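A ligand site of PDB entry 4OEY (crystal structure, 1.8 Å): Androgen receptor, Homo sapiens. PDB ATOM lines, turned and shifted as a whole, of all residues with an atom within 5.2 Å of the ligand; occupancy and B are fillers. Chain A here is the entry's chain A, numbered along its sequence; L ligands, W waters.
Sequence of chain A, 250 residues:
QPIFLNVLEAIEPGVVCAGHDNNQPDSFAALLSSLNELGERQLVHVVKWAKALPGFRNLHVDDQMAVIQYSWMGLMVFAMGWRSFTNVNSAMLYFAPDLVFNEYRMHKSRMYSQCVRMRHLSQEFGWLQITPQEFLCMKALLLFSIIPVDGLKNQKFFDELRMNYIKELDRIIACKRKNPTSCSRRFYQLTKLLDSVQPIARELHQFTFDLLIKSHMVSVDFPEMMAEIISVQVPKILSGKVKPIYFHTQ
NH2 of Arg 83 is in hydrogen-bond range of O1 of the ligand, at 2.9 Å. An oxygen (O1) of the ligand lies close to the side-chain amide oxygen (OE1) of Gln 42 (3.4 Å). An oxygen (O2) of the ligand lies within hydrogen-bond range of the side-chain hydroxyl (OG1) of Thr 208 (2.8 Å). The side-chain amide oxygen (OD1) of Asn 36 sits at hydrogen-bond distance from an oxygen (O2) of the ligand (2.5 Å).
Leu 32 touches the ligand (CD1 to C16, 3.7 Å). Leu 35 touches the ligand. Leu 38 touches the ligand (CD2 to C2, 3.9 Å). Met 73 touches the ligand (CE to C18, 3.7 Å). SD of Met 76 touches C19 of the ligand (3.6 Å). CB of Met 80 touches O1 of the ligand (3.6 Å). CD2 of Phe 95 touches O1 of the ligand, at 3.7 Å. Met 111 touches the ligand (SD to C15, 3.8 Å). CD1 of Phe 207 touches C16 of the ligand, at 3.9 Å. Phe 222 touches the ligand (CE2 to O2, 3.97 Å). Met 226 touches the ligand. Within 4 Å of the ligand: Leu 32, Leu 35, Asn 36, Leu 38, Gln 42, Met 73, Met 76, Met 80, Arg 83, Phe 95, Met 111, Phe 207, Thr 208, Phe 222 and Met 226.
Water W1 lies within hydrogen-bond range of the side-chain amide nitrogen of Gln 42, the backbone carbonyl oxygen of Met 76, the guanidinium group of Arg 83 and an oxygen (O1) of the ligand.
The guanidinium group (NH2) of Arg 83 lies within hydrogen-bond range of the backbone carbonyl oxygen (O) of Phe 95 (2.9 Å). The side-chain amide nitrogen (NE2) of Gln 42 lies close to the side-chain sulfur (SD) of Met 76 (3.6 Å). The guanidinium group (NH2) of Arg 83 is in hydrogen-bond range of the side-chain amide oxygen (OE1) of Gln 42 (3.3 Å).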
ATOM      1  N   LEU A  32      20.039  29.847  20.435  1.00  0.00           N
ATOM      2  CA  LEU A  32      19.917  29.546  19.051  1.00  0.00           C
ATOM      3  C   LEU A  32      20.949  30.311  18.263  1.00  0.00           C
ATOM      4  O   LEU A  32      21.514  29.748  17.301  1.00  0.00           O
ATOM      5  CB  LEU A  32      18.513  29.778  18.521  1.00  0.00           C
ATOM      6  CG  LEU A  32      17.505  28.626  18.481  1.00  0.00           C
ATOM      7  CD1 LEU A  32      17.898  27.481  17.540  1.00  0.00           C
ATOM      8  CD2 LEU A  32      17.310  28.172  19.911  1.00  0.00           C
ATOM      9  N   LEU A  35      24.003  28.125  18.601  1.00  0.00           N
ATOM     10  CA  LEU A  35      23.880  26.943  17.719  1.00  0.00           C
ATOM     11  C   LEU A  35      24.114  27.297  16.257  1.00  0.00           C
ATOM     12  O   LEU A  35      24.785  26.586  15.544  1.00  0.00           O
ATOM     13  CB  LEU A  35      22.514  26.283  17.918  1.00  0.00           C
ATOM     14  CG  LEU A  35      22.248  25.432  19.140  1.00  0.00           C
ATOM     15  CD1 LEU A  35      20.811  24.974  19.214  1.00  0.00           C
ATOM     16  CD2 LEU A  35      23.168  24.230  19.083  1.00  0.00           C
ATOM     17  N   ASN A  36      23.618  28.463  15.777  1.00  0.00           N
ATOM     18  CA  ASN A  36      23.844  28.892  14.398  1.00  0.00           C
ATOM     19  C   ASN A  36      25.328  29.160  14.120  1.00  0.00           C
ATOM     20  O   ASN A  36      25.828  28.775  13.104  1.00  0.00           O
ATOM     21  CB  ASN A  36      22.981  30.165  14.044  1.00  0.00           C
ATOM     22  CG  ASN A  36      21.482  29.848  13.918  1.00  0.00           C
ATOM     23  OD1 ASN A  36      21.084  28.665  13.711  1.00  0.00           O
ATOM     24  ND2 ASN A  36      20.623  30.883  14.068  1.00  0.00           N
ATOM     25  N   LEU A  38      27.743  27.815  15.784  1.00  0.00           N
ATOM     26  CA  LEU A  38      28.364  26.517  15.769  1.00  0.00           C
ATOM     27  C   LEU A  38      28.177  25.845  14.408  1.00  0.00           C
ATOM     28  O   LEU A  38      29.094  25.161  13.948  1.00  0.00           O
ATOM     29  CB  LEU A  38      27.729  25.607  16.923  1.00  0.00           C
ATOM     30  CG  LEU A  38      28.508  24.295  17.020  1.00  0.00           C
ATOM     31  CD1 LEU A  38      29.960  24.400  17.305  1.00  0.00           C
ATOM     32  CD2 LEU A  38      27.750  23.475  18.056  1.00  0.00           C
ATOM     33  N   GLY A  39      26.966  25.909  13.827  1.00  0.00           N
ATOM     34  CA  GLY A  39      26.659  25.313  12.539  1.00  0.00           C
ATOM     35  C   GLY A  39      27.642  25.898  11.505  1.00  0.00           C
ATOM     36  O   GLY A  39      28.195  25.246  10.682  1.00  0.00           O
ATOM     37  N   GLN A  42      31.208  24.523  12.247  1.00  0.00           N
ATOM     38  CA  GLN A  42      31.215  23.156  11.771  1.00  0.00           C
ATOM     39  C   GLN A  42      31.173  22.971  10.247  1.00  0.00           C
ATOM     40  O   GLN A  42      31.697  22.005   9.695  1.00  0.00           O
ATOM     41  CB  GLN A  42      30.156  22.242  12.494  1.00  0.00           C
ATOM     42  CG  GLN A  42      30.328  22.079  13.991  1.00  0.00           C
ATOM     43  CD  GLN A  42      29.519  20.945  14.629  1.00  0.00           C
ATOM     44  OE1 GLN A  42      29.510  20.771  15.863  1.00  0.00           O
ATOM     45  NE2 GLN A  42      28.780  20.219  13.808  1.00  0.00           N
ATOM     46  N   TRP A  72      24.630  18.341   5.356  1.00  0.00           N
ATOM     47  CA  TRP A  72      25.232  18.806   6.571  1.00  0.00           C
ATOM     48  C   TRP A  72      24.423  18.594   7.840  1.00  0.00           C
ATOM     49  O   TRP A  72      24.985  18.300   8.855  1.00  0.00           O
ATOM     50  CB  TRP A  72      25.689  20.340   6.468  1.00  0.00           C
ATOM     51  CG  TRP A  72      24.547  21.206   6.234  1.00  0.00           C
ATOM     52  CD1 TRP A  72      24.027  21.490   5.048  1.00  0.00           C
ATOM     53  CD2 TRP A  72      23.759  21.913   7.209  1.00  0.00           C
ATOM     54  NE1 TRP A  72      22.928  22.309   5.195  1.00  0.00           N
ATOM     55  CE2 TRP A  72      22.746  22.583   6.520  1.00  0.00           C
ATOM     56  CE3 TRP A  72      23.878  22.142   8.593  1.00  0.00           C
ATOM     57  CZ2 TRP A  72      21.789  23.351   7.151  1.00  0.00           C
ATOM     58  CZ3 TRP A  72      22.902  22.849   9.218  1.00  0.00           C
ATOM     59  CH2 TRP A  72      21.890  23.501   8.503  1.00  0.00           C
ATOM     60  N   MET A  73      23.104  18.748   7.808  1.00  0.00           N
ATOM     61  CA  MET A  73      22.299  18.670   8.988  1.00  0.00           C
ATOM     62  C   MET A  73      22.422  17.225   9.606  1.00  0.00           C
ATOM     63  O   MET A  73      22.669  17.082  10.791  1.00  0.00           O
ATOM     64  CB  MET A  73      20.875  19.030   8.692  1.00  0.00           C
ATOM     65  CG  MET A  73      19.987  19.045   9.922  1.00  0.00           C
ATOM     66  SD  MET A  73      20.266  20.322  11.134  1.00  0.00           S
ATOM     67  CE  MET A  73      19.369  21.626  10.301  1.00  0.00           C
ATOM     68  N   MET A  76      26.043  16.503  10.921  1.00  0.00           N
ATOM     69  CA  MET A  76      26.268  17.141  12.181  1.00  0.00           C
ATOM     70  C   MET A  76      25.508  16.538  13.364  1.00  0.00           C
ATOM     71  O   MET A  76      26.053  16.412  14.487  1.00  0.00           O
ATOM     72  CB  MET A  76      26.016  18.713  12.078  1.00  0.00           C
ATOM     73  CG  MET A  76      27.022  19.298  11.182  1.00  0.00           C
ATOM     74  SD  MET A  76      26.582  21.099  11.083  1.00  0.00           S
ATOM     75  CE  MET A  76      27.734  21.605   9.836  1.00  0.00           C
ATOM     76  N   VAL A  77      24.282  16.068  13.064  1.00  0.00           N
ATOM     77  CA  VAL A  77      23.399  15.635  14.075  1.00  0.00           C
ATOM     78  C   VAL A  77      23.995  14.264  14.537  1.00  0.00           C
ATOM     79  O   VAL A  77      23.987  13.992  15.715  1.00  0.00           O
ATOM     80  CB  VAL A  77      21.960  15.473  13.537  1.00  0.00           C
ATOM     81  CG1 VAL A  77      21.138  14.507  14.409  1.00  0.00           C
ATOM     82  CG2 VAL A  77      21.209  16.815  13.580  1.00  0.00           C
ATOM     83  N   MET A  80      27.054  14.780  16.493  1.00  0.00           N
ATOM     84  CA  MET A  80      26.749  15.289  17.814  1.00  0.00           C
ATOM     85  C   MET A  80      26.202  14.162  18.724  1.00  0.00           C
ATOM     86  O   MET A  80      26.551  14.082  19.911  1.00  0.00           O
ATOM     87  CB  MET A  80      25.726  16.367  17.719  1.00  0.00           C
ATOM     88  CG  MET A  80      25.474  17.030  19.065  1.00  0.00           C
ATOM     89  SD  MET A  80      24.120  16.310  20.021  1.00  0.00           S
ATOM     90  CE  MET A  80      22.763  16.426  18.914  1.00  0.00           C
ATOM     91  N   ARG A  83      29.265  12.225  19.993  1.00  0.00           N
ATOM     92  CA  ARG A  83      29.956  12.967  21.045  1.00  0.00           C
ATOM     93  C   ARG A  83      29.182  12.923  22.344  1.00  0.00           C
ATOM     94  O   ARG A  83      29.785  12.950  23.451  1.00  0.00           O
ATOM     95  CB  ARG A  83      30.037  14.484  20.665  1.00  0.00           C
ATOM     96  CG  ARG A  83      30.948  14.872  19.543  1.00  0.00           C
ATOM     97  CD  ARG A  83      31.244  16.394  19.555  1.00  0.00           C
ATOM     98  NE  ARG A  83      30.093  17.214  19.176  1.00  0.00           N
ATOM     99  CZ  ARG A  83      29.688  17.406  17.932  1.00  0.00           C
ATOM    100  NH1 ARG A  83      30.303  16.849  16.911  1.00  0.00           N
ATOM    101  NH2 ARG A  83      28.649  18.223  17.710  1.00  0.00           N
ATOM    102  N   PHE A  95      26.616  19.420  21.961  1.00  0.00           N
ATOM    103  CA  PHE A  95      26.845  20.157  20.715  1.00  0.00           C
ATOM    104  C   PHE A  95      28.308  20.560  20.616  1.00  0.00           C
ATOM    105  O   PHE A  95      28.940  20.396  19.582  1.00  0.00           O
ATOM    106  CB  PHE A  95      25.908  21.326  20.634  1.00  0.00           C
ATOM    107  CG  PHE A  95      24.458  20.966  20.545  1.00  0.00           C
ATOM    108  CD1 PHE A  95      23.645  21.176  21.613  1.00  0.00           C
ATOM    109  CD2 PHE A  95      23.909  20.526  19.348  1.00  0.00           C
ATOM    110  CE1 PHE A  95      22.269  20.897  21.529  1.00  0.00           C
ATOM    111  CE2 PHE A  95      22.547  20.230  19.291  1.00  0.00           C
ATOM    112  CZ  PHE A  95      21.759  20.404  20.361  1.00  0.00           C
ATOM    113  N   MET A 111      12.856  23.595  20.976  1.00  0.00           N
ATOM    114  CA  MET A 111      13.168  22.501  20.087  1.00  0.00           C
ATOM    115  C   MET A 111      13.191  21.255  20.944  1.00  0.00           C
ATOM    116  O   MET A 111      13.935  20.296  20.670  1.00  0.00           O
ATOM    117  CB  MET A 111      14.604  22.553  19.584  1.00  0.00           C
ATOM    118  CG  MET A 111      14.937  23.650  18.633  1.00  0.00           C
ATOM    119  SD  MET A 111      16.423  23.069  17.798  1.00  0.00           S
ATOM    120  CE  MET A 111      17.698  23.574  18.925  1.00  0.00           C
ATOM    121  N   MET A 118      17.099  13.645  19.137  1.00  0.00           N
ATOM    122  CA  MET A 118      18.537  13.536  19.032  1.00  0.00           C
ATOM    123  C   MET A 118      19.127  12.766  20.223  1.00  0.00           C
ATOM    124  O   MET A 118      20.134  12.024  20.099  1.00  0.00           O
ATOM    125  CB  MET A 118      19.162  14.952  18.893  1.00  0.00           C
ATOM    126  CG  MET A 118      18.668  15.647  17.649  1.00  0.00           C
ATOM    127  SD  MET A 118      19.653  17.129  17.356  1.00  0.00           S
ATOM    128  CE  MET A 118      18.834  18.331  18.348  1.00  0.00           C
ATOM    129  N   LEU A 204      14.496  19.276  12.036  1.00  0.00           N
ATOM    130  CA  LEU A 204      15.464  20.401  12.184  1.00  0.00           C
ATOM    131  C   LEU A 204      15.486  21.341  10.990  1.00  0.00           C
ATOM    132  O   LEU A 204      15.619  22.584  11.179  1.00  0.00           O
ATOM    133  CB  LEU A 204      16.854  19.853  12.498  1.00  0.00           C
ATOM    134  CG  LEU A 204      16.919  19.173  13.910  1.00  0.00           C
ATOM    135  CD1 LEU A 204      18.200  18.470  14.153  1.00  0.00           C
ATOM    136  CD2 LEU A 204      16.673  20.126  15.041  1.00  0.00           C
ATOM    137  N   PHE A 207      12.424  23.441  11.372  1.00  0.00           N
ATOM    138  CA  PHE A 207      12.621  24.393  12.480  1.00  0.00           C
ATOM    139  C   PHE A 207      13.527  25.553  12.061  1.00  0.00           C
ATOM    140  O   PHE A 207      13.201  26.776  12.299  1.00  0.00           O
ATOM    141  CB  PHE A 207      13.254  23.702  13.683  1.00  0.00           C
ATOM    142  CG  PHE A 207      13.238  24.533  14.931  1.00  0.00           C
ATOM    143  CD1 PHE A 207      14.325  25.305  15.270  1.00  0.00           C
ATOM    144  CD2 PHE A 207      12.123  24.569  15.740  1.00  0.00           C
ATOM    145  CE1 PHE A 207      14.324  26.086  16.418  1.00  0.00           C
ATOM    146  CE2 PHE A 207      12.102  25.356  16.895  1.00  0.00           C
ATOM    147  CZ  PHE A 207      13.202  26.133  17.224  1.00  0.00           C
ATOM    148  N   THR A 208      14.647  25.220  11.449  1.00  0.00           N
ATOM    149  CA  THR A 208      15.683  26.283  11.162  1.00  0.00           C
ATOM    150  C   THR A 208      15.142  27.170  10.058  1.00  0.00           C
ATOM    151  O   THR A 208      15.331  28.383  10.093  1.00  0.00           O
ATOM    152  CB  THR A 208      17.095  25.722  10.836  1.00  0.00           C
ATOM    153  OG1 THR A 208      18.088  26.762  10.916  1.00  0.00           O
ATOM    154  CG2 THR A 208      17.175  25.123   9.478  1.00  0.00           C
ATOM    155  N   LEU A 211      12.692  29.489  11.724  1.00  0.00           N
ATOM    156  CA  LEU A 211      13.480  30.415  12.505  1.00  0.00           C
ATOM    157  C   LEU A 211      14.162  31.460  11.630  1.00  0.00           C
ATOM    158  O   LEU A 211      14.226  32.632  12.020  1.00  0.00           O
ATOM    159  CB  LEU A 211      14.536  29.704  13.355  1.00  0.00           C
ATOM    160  CG  LEU A 211      15.304  30.566  14.360  1.00  0.00           C
ATOM    161  CD1 LEU A 211      14.416  31.378  15.297  1.00  0.00           C
ATOM    162  CD2 LEU A 211      16.214  29.697  15.179  1.00  0.00           C
ATOM    163  N   PHE A 222      21.620  34.716  12.294  1.00  0.00           N
ATOM    164  CA  PHE A 222      22.188  33.707  11.363  1.00  0.00           C
ATOM    165  C   PHE A 222      23.402  34.226  10.659  1.00  0.00           C
ATOM    166  O   PHE A 222      23.315  35.240   9.913  1.00  0.00           O
ATOM    167  CB  PHE A 222      21.207  33.243  10.302  1.00  0.00           C
ATOM    168  CG  PHE A 222      20.101  32.356  10.805  1.00  0.00           C
ATOM    169  CD1 PHE A 222      19.062  32.887  11.515  1.00  0.00           C
ATOM    170  CD2 PHE A 222      20.052  30.982  10.504  1.00  0.00           C
ATOM    171  CE1 PHE A 222      17.991  32.119  11.978  1.00  0.00           C
ATOM    172  CE2 PHE A 222      18.983  30.209  10.947  1.00  0.00           C
ATOM    173  CZ  PHE A 222      17.945  30.755  11.674  1.00  0.00           C
ATOM    174  N   MET A 226      25.155  30.072   6.680  1.00  0.00           N
ATOM    175  CA  MET A 226      23.933  29.424   7.200  1.00  0.00           C
ATOM    176  C   MET A 226      22.659  30.062   6.591  1.00  0.00           C
ATOM    177  O   MET A 226      21.758  29.356   6.166  1.00  0.00           O
ATOM    178  CB  MET A 226      23.890  29.422   8.748  1.00  0.00           C
ATOM    179  CG  MET A 226      24.932  28.504   9.436  1.00  0.00           C
ATOM    180  SD  MET A 226      24.557  26.707   9.358  1.00  0.00           S
ATOM    181  CE  MET A 226      23.094  26.623  10.327  1.00  0.00           C
ATOM    182  N   ILE A 230      20.230  27.830   4.112  1.00  0.00           N
ATOM    183  CA  ILE A 230      18.885  27.606   4.630  1.00  0.00           C
ATOM    184  C   ILE A 230      17.840  28.347   3.741  1.00  0.00           C
ATOM    185  O   ILE A 230      16.744  27.939   3.623  1.00  0.00           O
ATOM    186  CB  ILE A 230      18.787  28.007   6.104  1.00  0.00           C
ATOM    187  CG1 ILE A 230      19.867  27.260   6.956  1.00  0.00           C
ATOM    188  CG2 ILE A 230      17.338  27.855   6.655  1.00  0.00           C
ATOM    189  CD1 ILE A 230      20.031  27.769   8.360  1.00  0.00           C
HETATM  190  C1  LIG L   1      25.016  22.525  15.040  1.00  0.00           C
HETATM  191  C2  LIG L   1      26.144  21.500  15.099  1.00  0.00           C
HETATM  192  C3  LIG L   1      25.664  20.306  15.887  1.00  0.00           C
HETATM  193  O1  LIG L   1      26.398  19.805  16.724  1.00  0.00           O
HETATM  194  C4  LIG L   1      24.218  19.918  15.650  1.00  0.00           C
HETATM  195  C5  LIG L   1      23.236  21.048  15.627  1.00  0.00           C
HETATM  196  C6  LIG L   1      21.816  20.506  15.383  1.00  0.00           C
HETATM  197  C7  LIG L   1      20.785  21.626  15.484  1.00  0.00           C
HETATM  198  C8  LIG L   1      21.097  22.763  14.509  1.00  0.00           C
HETATM  199  C9  LIG L   1      22.558  23.195  14.683  1.00  0.00           C
HETATM  200  C10 LIG L   1      23.600  22.120  14.561  1.00  0.00           C
HETATM  201  C11 LIG L   1      22.937  24.405  13.758  1.00  0.00           C
HETATM  202  C12 LIG L   1      21.875  25.516  13.921  1.00  0.00           C
HETATM  203  C13 LIG L   1      20.427  25.055  13.766  1.00  0.00           C
HETATM  204  C14 LIG L   1      20.183  23.938  14.793  1.00  0.00           C
HETATM  205  C15 LIG L   1      18.656  23.778  14.767  1.00  0.00           C
HETATM  206  C16 LIG L   1      18.140  25.232  14.570  1.00  0.00           C
HETATM  207  C17 LIG L   1      19.416  26.058  14.328  1.00  0.00           C
HETATM  208  O2  LIG L   1      19.049  27.174  13.509  1.00  0.00           O
HETATM  209  C18 LIG L   1      20.156  24.625  12.341  1.00  0.00           C
HETATM  210  C19 LIG L   1      23.664  21.545  13.122  1.00  0.00           C
HETATM  211  O   HOH W   1      28.360  17.989  14.824  1.00  0.00           O
